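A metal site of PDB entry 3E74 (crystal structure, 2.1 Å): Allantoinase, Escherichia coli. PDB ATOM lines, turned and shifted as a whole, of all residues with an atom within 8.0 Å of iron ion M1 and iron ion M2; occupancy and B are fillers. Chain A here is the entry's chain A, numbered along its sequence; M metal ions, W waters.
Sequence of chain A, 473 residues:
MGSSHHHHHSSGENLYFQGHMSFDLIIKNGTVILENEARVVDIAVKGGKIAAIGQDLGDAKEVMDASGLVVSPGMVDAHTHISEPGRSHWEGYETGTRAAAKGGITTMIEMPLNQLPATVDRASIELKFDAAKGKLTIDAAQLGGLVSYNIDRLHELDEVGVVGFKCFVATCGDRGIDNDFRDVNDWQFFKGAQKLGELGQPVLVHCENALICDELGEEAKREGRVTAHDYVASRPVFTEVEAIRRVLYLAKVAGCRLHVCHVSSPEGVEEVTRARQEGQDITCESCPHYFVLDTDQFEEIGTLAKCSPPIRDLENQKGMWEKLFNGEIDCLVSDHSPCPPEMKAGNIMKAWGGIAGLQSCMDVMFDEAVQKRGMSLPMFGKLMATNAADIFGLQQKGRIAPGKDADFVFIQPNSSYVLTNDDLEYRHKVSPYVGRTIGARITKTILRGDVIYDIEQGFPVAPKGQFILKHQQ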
ATOM      1  N   HIS A  79      28.529  17.340  10.486  1.00  0.00           N
ATOM      2  CA  HIS A  79      27.390  17.080  11.349  1.00  0.00           C
ATOM      3  C   HIS A  79      26.601  15.826  10.976  1.00  0.00           C
ATOM      4  O   HIS A  79      25.528  15.887  10.364  1.00  0.00           O
ATOM      5  CB  HIS A  79      26.468  18.296  11.342  1.00  0.00           C
ATOM      6  CG  HIS A  79      25.412  18.267  12.400  1.00  0.00           C
ATOM      7  ND1 HIS A  79      24.870  19.409  12.943  1.00  0.00           N
ATOM      8  CD2 HIS A  79      24.788  17.225  13.004  1.00  0.00           C
ATOM      9  CE1 HIS A  79      23.949  19.078  13.831  1.00  0.00           C
ATOM     10  NE2 HIS A  79      23.871  17.750  13.881  1.00  0.00           N
ATOM     11  N   THR A  80      27.123  14.665  11.376  1.00  0.00           N
ATOM     12  CA  THR A  80      26.424  13.440  11.067  1.00  0.00           C
ATOM     13  C   THR A  80      26.197  12.521  12.267  1.00  0.00           C
ATOM     14  O   THR A  80      27.025  12.426  13.174  1.00  0.00           O
ATOM     15  CB  THR A  80      27.129  12.690   9.889  1.00  0.00           C
ATOM     16  OG1 THR A  80      26.987  11.276  10.057  1.00  0.00           O
ATOM     17  CG2 THR A  80      28.565  13.081   9.780  1.00  0.00           C
ATOM     18  N   HIS A  81      25.034  11.880  12.270  1.00  0.00           N
ATOM     19  CA  HIS A  81      24.664  10.953  13.340  1.00  0.00           C
ATOM     20  C   HIS A  81      24.713   9.534  12.785  1.00  0.00           C
ATOM     21  O   HIS A  81      24.092   9.233  11.772  1.00  0.00           O
ATOM     22  CB  HIS A  81      23.270  11.269  13.852  1.00  0.00           C
ATOM     23  CG  HIS A  81      23.146  12.652  14.444  1.00  0.00           C
ATOM     24  ND1 HIS A  81      23.554  12.951  15.724  1.00  0.00           N
ATOM     25  CD2 HIS A  81      22.690  13.804  13.905  1.00  0.00           C
ATOM     26  CE1 HIS A  81      23.356  14.244  15.950  1.00  0.00           C
ATOM     27  NE2 HIS A  81      22.841  14.780  14.863  1.00  0.00           N
ATOM     28  N   MET A 111      28.843  13.025  15.607  1.00  0.00           N
ATOM     29  CA  MET A 111      28.207  13.624  16.768  1.00  0.00           C
ATOM     30  C   MET A 111      28.304  12.664  17.943  1.00  0.00           C
ATOM     31  O   MET A 111      28.284  11.452  17.759  1.00  0.00           O
ATOM     32  CB  MET A 111      26.752  13.953  16.463  1.00  0.00           C
ATOM     33  CG  MET A 111      26.587  15.175  15.560  1.00  0.00           C
ATOM     34  SD  MET A 111      26.929  16.836  16.522  1.00  0.00           S
ATOM     35  CE  MET A 111      27.347  18.021  15.036  1.00  0.00           C
ATOM     36  N   LEU A 113      26.296  12.839  21.385  1.00  0.00           N
ATOM     37  CA  LEU A 113      25.068  12.466  22.071  1.00  0.00           C
ATOM     38  C   LEU A 113      24.128  11.600  21.226  1.00  0.00           C
ATOM     39  O   LEU A 113      24.404  11.361  20.051  1.00  0.00           O
ATOM     40  CB  LEU A 113      24.348  13.738  22.567  1.00  0.00           C
ATOM     41  CG  LEU A 113      24.947  14.413  23.816  1.00  0.00           C
ATOM     42  CD1 LEU A 113      26.382  14.810  23.557  1.00  0.00           C
ATOM     43  CD2 LEU A 113      24.136  15.641  24.175  1.00  0.00           C
ATOM     44  N   ASN A 114      23.051  11.133  21.854  1.00  0.00           N
ATOM     45  CA  ASN A 114      22.064  10.277  21.194  1.00  0.00           C
ATOM     46  C   ASN A 114      22.720   9.073  20.515  1.00  0.00           C
ATOM     47  O   ASN A 114      22.583   8.851  19.310  1.00  0.00           O
ATOM     48  CB  ASN A 114      21.251  11.079  20.169  1.00  0.00           C
ATOM     49  CG  ASN A 114      20.327  12.090  20.828  1.00  0.00           C
ATOM     50  OD1 ASN A 114      19.371  11.716  21.518  1.00  0.00           O
ATOM     51  ND2 ASN A 114      20.619  13.378  20.648  1.00  0.00           N
ATOM     52  N   KCX A 166      29.882  19.026  21.277  1.00  0.00           N
ATOM     53  CA  KCX A 166      28.492  19.370  21.024  1.00  0.00           C
ATOM     54  CB  KCX A 166      27.870  18.334  20.097  1.00  0.00           C
ATOM     55  CG  KCX A 166      26.933  18.866  19.033  1.00  0.00           C
ATOM     56  CD  KCX A 166      25.678  19.469  19.595  1.00  0.00           C
ATOM     57  CE  KCX A 166      24.654  19.748  18.497  1.00  0.00           C
ATOM     58  NZ  KCX A 166      24.136  18.518  17.881  1.00  0.00           N
ATOM     59  C   KCX A 166      27.685  19.438  22.330  1.00  0.00           C
ATOM     60  O   KCX A 166      27.938  18.677  23.270  1.00  0.00           O
ATOM     61  CX  KCX A 166      22.975  18.426  17.229  1.00  0.00           C
ATOM     62  OQ1 KCX A 166      22.636  17.320  16.743  1.00  0.00           O
ATOM     63  OQ2 KCX A 166      22.248  19.448  17.139  1.00  0.00           O
ATOM     64  N   CYS A 167      26.708  20.353  22.378  1.00  0.00           N
ATOM     65  CA  CYS A 167      25.842  20.479  23.544  1.00  0.00           C
ATOM     66  C   CYS A 167      24.502  21.099  23.144  1.00  0.00           C
ATOM     67  O   CYS A 167      24.383  21.730  22.074  1.00  0.00           O
ATOM     68  CB  CYS A 167      26.492  21.327  24.631  1.00  0.00           C
ATOM     69  SG  CYS A 167      26.520  23.091  24.291  1.00  0.00           S
ATOM     70  N   PHE A 168      23.498  20.898  23.994  1.00  0.00           N
ATOM     71  CA  PHE A 168      22.178  21.433  23.734  1.00  0.00           C
ATOM     72  C   PHE A 168      21.780  22.445  24.782  1.00  0.00           C
ATOM     73  O   PHE A 168      21.858  22.175  25.991  1.00  0.00           O
ATOM     74  CB  PHE A 168      21.148  20.299  23.673  1.00  0.00           C
ATOM     75  CG  PHE A 168      21.397  19.308  22.586  1.00  0.00           C
ATOM     76  CD1 PHE A 168      22.472  18.424  22.659  1.00  0.00           C
ATOM     77  CD2 PHE A 168      20.602  19.303  21.437  1.00  0.00           C
ATOM     78  CE1 PHE A 168      22.755  17.552  21.608  1.00  0.00           C
ATOM     79  CE2 PHE A 168      20.884  18.425  20.378  1.00  0.00           C
ATOM     80  CZ  PHE A 168      21.951  17.549  20.459  1.00  0.00           C
ATOM     81  N   VAL A 205      26.751  24.218  19.141  1.00  0.00           N
ATOM     82  CA  VAL A 205      25.466  24.269  19.815  1.00  0.00           C
ATOM     83  C   VAL A 205      24.210  24.207  18.951  1.00  0.00           C
ATOM     84  O   VAL A 205      24.119  24.868  17.917  1.00  0.00           O
ATOM     85  CB  VAL A 205      25.330  25.557  20.694  1.00  0.00           C
ATOM     86  CG1 VAL A 205      24.063  25.486  21.509  1.00  0.00           C
ATOM     87  CG2 VAL A 205      26.541  25.752  21.597  1.00  0.00           C
ATOM     88  N   HIS A 206      23.247  23.404  19.422  1.00  0.00           N
ATOM     89  CA  HIS A 206      21.924  23.264  18.805  1.00  0.00           C
ATOM     90  C   HIS A 206      21.127  24.440  19.415  1.00  0.00           C
ATOM     91  O   HIS A 206      20.737  24.378  20.583  1.00  0.00           O
ATOM     92  CB  HIS A 206      21.271  21.933  19.231  1.00  0.00           C
ATOM     93  CG  HIS A 206      19.874  21.778  18.734  1.00  0.00           C
ATOM     94  ND1 HIS A 206      19.535  20.897  17.729  1.00  0.00           N
ATOM     95  CD2 HIS A 206      18.738  22.454  19.032  1.00  0.00           C
ATOM     96  CE1 HIS A 206      18.252  21.039  17.426  1.00  0.00           C
ATOM     97  NE2 HIS A 206      17.753  21.984  18.194  1.00  0.00           N
ATOM     98  N   CYS A 207      20.882  25.495  18.651  1.00  0.00           N
ATOM     99  CA  CYS A 207      20.214  26.674  19.202  1.00  0.00           C
ATOM    100  C   CYS A 207      18.723  26.896  18.963  1.00  0.00           C
ATOM    101  O   CYS A 207      18.336  27.520  17.967  1.00  0.00           O
ATOM    102  CB  CYS A 207      20.964  27.941  18.754  1.00  0.00           C
ATOM    103  SG  CYS A 207      22.719  27.989  19.169  1.00  0.00           S
ATOM    104  N   GLU A 208      17.903  26.422  19.896  1.00  0.00           N
ATOM    105  CA  GLU A 208      16.439  26.601  19.890  1.00  0.00           C
ATOM    106  C   GLU A 208      15.975  26.682  21.339  1.00  0.00           C
ATOM    107  O   GLU A 208      16.510  25.975  22.222  1.00  0.00           O
ATOM    108  CB  GLU A 208      15.712  25.410  19.281  1.00  0.00           C
ATOM    109  CG  GLU A 208      15.616  25.374  17.771  1.00  0.00           C
ATOM    110  CD  GLU A 208      14.757  24.219  17.305  1.00  0.00           C
ATOM    111  OE1 GLU A 208      15.074  23.062  17.651  1.00  0.00           O
ATOM    112  OE2 GLU A 208      13.754  24.488  16.589  1.00  0.00           O
ATOM    113  N   CYS A 261      25.035  25.392  15.104  1.00  0.00           N
ATOM    114  CA  CYS A 261      24.497  24.276  14.316  1.00  0.00           C
ATOM    115  C   CYS A 261      23.221  24.567  13.519  1.00  0.00           C
ATOM    116  O   CYS A 261      22.407  25.444  13.873  1.00  0.00           O
ATOM    117  CB  CYS A 261      24.274  23.055  15.232  1.00  0.00           C
ATOM    118  SG  CYS A 261      25.810  22.171  15.731  1.00  0.00           S
ATOM    119  N   HIS A 262      23.096  23.852  12.403  1.00  0.00           N
ATOM    120  CA  HIS A 262      21.948  23.930  11.499  1.00  0.00           C
ATOM    121  C   HIS A 262      21.048  25.180  11.673  1.00  0.00           C
ATOM    122  O   HIS A 262      20.002  25.119  12.324  1.00  0.00           O
ATOM    123  CB  HIS A 262      21.126  22.658  11.681  1.00  0.00           C
ATOM    124  CG  HIS A 262      20.856  22.315  13.118  1.00  0.00           C
ATOM    125  ND1 HIS A 262      20.396  23.237  14.030  1.00  0.00           N
ATOM    126  CD2 HIS A 262      20.940  21.131  13.789  1.00  0.00           C
ATOM    127  CE1 HIS A 262      20.198  22.644  15.198  1.00  0.00           C
ATOM    128  NE2 HIS A 262      20.522  21.370  15.073  1.00  0.00           N
ATOM    129  N   GLU A 285      26.520  26.838  10.326  1.00  0.00           N
ATOM    130  CA  GLU A 285      26.265  25.911   9.228  1.00  0.00           C
ATOM    131  C   GLU A 285      24.761  25.855   8.974  1.00  0.00           C
ATOM    132  O   GLU A 285      23.979  26.423   9.727  1.00  0.00           O
ATOM    133  CB  GLU A 285      26.692  24.512   9.648  1.00  0.00           C
ATOM    134  CG  GLU A 285      25.892  24.050  10.886  1.00  0.00           C
ATOM    135  CD  GLU A 285      26.263  22.660  11.430  1.00  0.00           C
ATOM    136  OE1 GLU A 285      27.451  22.255  11.366  1.00  0.00           O
ATOM    137  OE2 GLU A 285      25.346  21.978  11.946  1.00  0.00           O
ATOM    138  N   CYS A 287      21.827  23.157   6.442  1.00  0.00           N
ATOM    139  CA  CYS A 287      21.735  21.872   5.757  1.00  0.00           C
ATOM    140  C   CYS A 287      20.940  21.982   4.468  1.00  0.00           C
ATOM    141  O   CYS A 287      20.116  22.886   4.328  1.00  0.00           O
ATOM    142  CB  CYS A 287      21.045  20.872   6.684  1.00  0.00           C
ATOM    143  SG  CYS A 287      21.591  21.005   8.397  1.00  0.00           S
ATOM    144  N   TYR A 290      17.118  22.939   4.255  1.00  0.00           N
ATOM    145  CA  TYR A 290      16.638  24.301   4.480  1.00  0.00           C
ATOM    146  C   TYR A 290      16.795  25.150   3.204  1.00  0.00           C
ATOM    147  O   TYR A 290      16.297  26.274   3.131  1.00  0.00           O
ATOM    148  CB  TYR A 290      17.418  24.970   5.630  1.00  0.00           C
ATOM    149  CG  TYR A 290      17.287  24.242   6.942  1.00  0.00           C
ATOM    150  CD1 TYR A 290      16.067  24.162   7.609  1.00  0.00           C
ATOM    151  CD2 TYR A 290      18.394  23.608   7.510  1.00  0.00           C
ATOM    152  CE1 TYR A 290      15.950  23.467   8.834  1.00  0.00           C
ATOM    153  CE2 TYR A 290      18.289  22.915   8.707  1.00  0.00           C
ATOM    154  CZ  TYR A 290      17.072  22.843   9.369  1.00  0.00           C
ATOM    155  OH  TYR A 290      16.973  22.130  10.542  1.00  0.00           O
ATOM    156  N   CYS A 307      12.027  17.835  10.988  1.00  0.00           N
ATOM    157  CA  CYS A 307      13.324  17.964  11.666  1.00  0.00           C
ATOM    158  C   CYS A 307      13.269  19.097  12.686  1.00  0.00           C
ATOM    159  O   CYS A 307      12.429  19.991  12.580  1.00  0.00           O
ATOM    160  CB  CYS A 307      14.447  18.224  10.672  1.00  0.00           C
ATOM    161  SG  CYS A 307      14.099  19.606   9.604  1.00  0.00           S
ATOM    162  N   SER A 308      14.175  19.063  13.660  1.00  0.00           N
ATOM    163  CA  SER A 308      14.187  20.045  14.735  1.00  0.00           C
ATOM    164  C   SER A 308      14.109  21.482  14.269  1.00  0.00           C
ATOM    165  O   SER A 308      13.000  22.020  14.218  1.00  0.00           O
ATOM    166  CB  SER A 308      15.376  19.833  15.651  1.00  0.00           C
ATOM    167  OG  SER A 308      15.045  20.284  16.948  1.00  0.00           O
ATOM    168  N   PRO A 309      15.244  22.157  13.967  1.00  0.00           N
ATOM    169  CA  PRO A 309      14.900  23.515  13.514  1.00  0.00           C
ATOM    170  C   PRO A 309      14.030  23.122  12.311  1.00  0.00           C
ATOM    171  O   PRO A 309      14.486  22.363  11.460  1.00  0.00           O
ATOM    172  CB  PRO A 309      16.251  24.126  13.122  1.00  0.00           C
ATOM    173  CG  PRO A 309      17.234  23.324  13.875  1.00  0.00           C
ATOM    174  CD  PRO A 309      16.681  21.899  13.800  1.00  0.00           C
ATOM    175  N   VAL A 333      26.046  21.050   6.031  1.00  0.00           N
ATOM    176  CA  VAL A 333      26.220  19.740   6.626  1.00  0.00           C
ATOM    177  C   VAL A 333      24.905  18.985   6.439  1.00  0.00           C
ATOM    178  O   VAL A 333      23.877  19.573   6.108  1.00  0.00           O
ATOM    179  CB  VAL A 333      26.595  19.834   8.137  1.00  0.00           C
ATOM    180  CG1 VAL A 333      27.918  20.612   8.307  1.00  0.00           C
ATOM    181  CG2 VAL A 333      25.491  20.521   8.936  1.00  0.00           C
ATOM    182  N   SER A 334      24.933  17.686   6.648  1.00  0.00           N
ATOM    183  CA  SER A 334      23.739  16.879   6.464  1.00  0.00           C
ATOM    184  C   SER A 334      22.806  16.794   7.662  1.00  0.00           C
ATOM    185  O   SER A 334      21.594  16.746   7.501  1.00  0.00           O
ATOM    186  CB  SER A 334      24.163  15.452   6.109  1.00  0.00           C
ATOM    187  OG  SER A 334      24.675  14.814   7.266  1.00  0.00           O
ATOM    188  N   ASP A 335      23.366  16.793   8.866  1.00  0.00           N
ATOM    189  CA  ASP A 335      22.556  16.566  10.068  1.00  0.00           C
ATOM    190  C   ASP A 335      21.792  15.243   9.823  1.00  0.00           C
ATOM    191  O   ASP A 335      20.632  15.081  10.232  1.00  0.00           O
ATOM    192  CB  ASP A 335      21.550  17.696  10.377  1.00  0.00           C
ATOM    193  CG  ASP A 335      20.907  17.531  11.778  1.00  0.00           C
ATOM    194  OD1 ASP A 335      21.466  16.790  12.607  1.00  0.00           O
ATOM    195  OD2 ASP A 335      19.840  18.122  12.062  1.00  0.00           O
ATOM    196  N   HIS A 336      22.439  14.315   9.129  1.00  0.00           N
ATOM    197  CA  HIS A 336      21.833  13.021   8.839  1.00  0.00           C
ATOM    198  C   HIS A 336      21.313  12.422  10.126  1.00  0.00           C
ATOM    199  O   HIS A 336      22.065  12.227  11.088  1.00  0.00           O
ATOM    200  CB  HIS A 336      22.844  12.089   8.187  1.00  0.00           C
ATOM    201  CG  HIS A 336      22.286  10.744   7.851  1.00  0.00           C
ATOM    202  ND1 HIS A 336      21.216  10.572   6.994  1.00  0.00           N
ATOM    203  CD2 HIS A 336      22.680   9.500   8.219  1.00  0.00           C
ATOM    204  CE1 HIS A 336      20.980   9.277   6.841  1.00  0.00           C
ATOM    205  NE2 HIS A 336      21.859   8.607   7.569  1.00  0.00           N
ATOM    206  N   SER A 337      20.013  12.155  10.152  1.00  0.00           N
ATOM    207  CA  SER A 337      19.378  11.609  11.336  1.00  0.00           C
ATOM    208  C   SER A 337      18.332  10.571  10.943  1.00  0.00           C
ATOM    209  O   SER A 337      17.142  10.871  10.810  1.00  0.00           O
ATOM    210  CB  SER A 337      18.724  12.736  12.139  1.00  0.00           C
ATOM    211  OG  SER A 337      18.164  12.231  13.343  1.00  0.00           O
HETATM  212 FE    FE M   1      20.290  19.337  16.386  1.00  0.00          FE
HETATM  213 FE    FE M   2      21.982  16.839  14.822  1.00  0.00          FE
HETATM  214  O   HOH W   1      19.726  16.391  17.007  1.00  0.00           O
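Of the 26 residues printed, 4 come within 4 Å of iron ion M2.
The nearest printed residue that does not touch iron ion M2 is His 262 (4.5 Å).
Iron ion M1 is bound by OQ2 of KCX 166 (2.1 Å), ND1 of His 206 (2.2 Å) and NE2 of His 262 (2.4 Å).
Iron ion M1 has three donor atoms within binding distance.
Three residues have an atom within 4 Å of iron ion M1: KCX 166, His 206 and His 262.
The nearest printed residue that does not touch iron ion M1 is Phe 168 (4.1 Å).
OQ1 of KCX 166 binds iron ion M2 (2.1 Å).
NE2 of His 81 binds iron ion M2, at 2.2 Å.
OD1 of Asp 335 is bound to iron ion M2 (2.3 Å).
Iron ion M2 is bound by NE2 of His 79, at 2.3 Å.
The side-chain sulfur (SD) of Met 111 sits close to NZ of KCX 166 (3.5 Å).
A ring nitrogen (NE2) of His 206 lies close to the side-chain hydroxyl of Ser 308 (3.4 Å).
NE2 of His 206 lies within hydrogen-bond range of OE1 of Glu 208 (2.9 Å).
N of His 206 sits at hydrogen-bond distance from O of Cys 167 (3.3 Å).
O of His 336 sits close to N of His 81 (3.2 Å).
OE2 of Glu 285 lies within hydrogen-bond range of ND1 of His 79 (2.8 Å).
The backbone carbonyl oxygen (O) of His 79 sits at hydrogen-bond distance from the side-chain hydroxyl (OG) of Ser 334 (3.4 Å).
The backbone NH of His 262 is in hydrogen-bond range of the side-chain carboxylate of Glu 285, 3.0 Å away.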
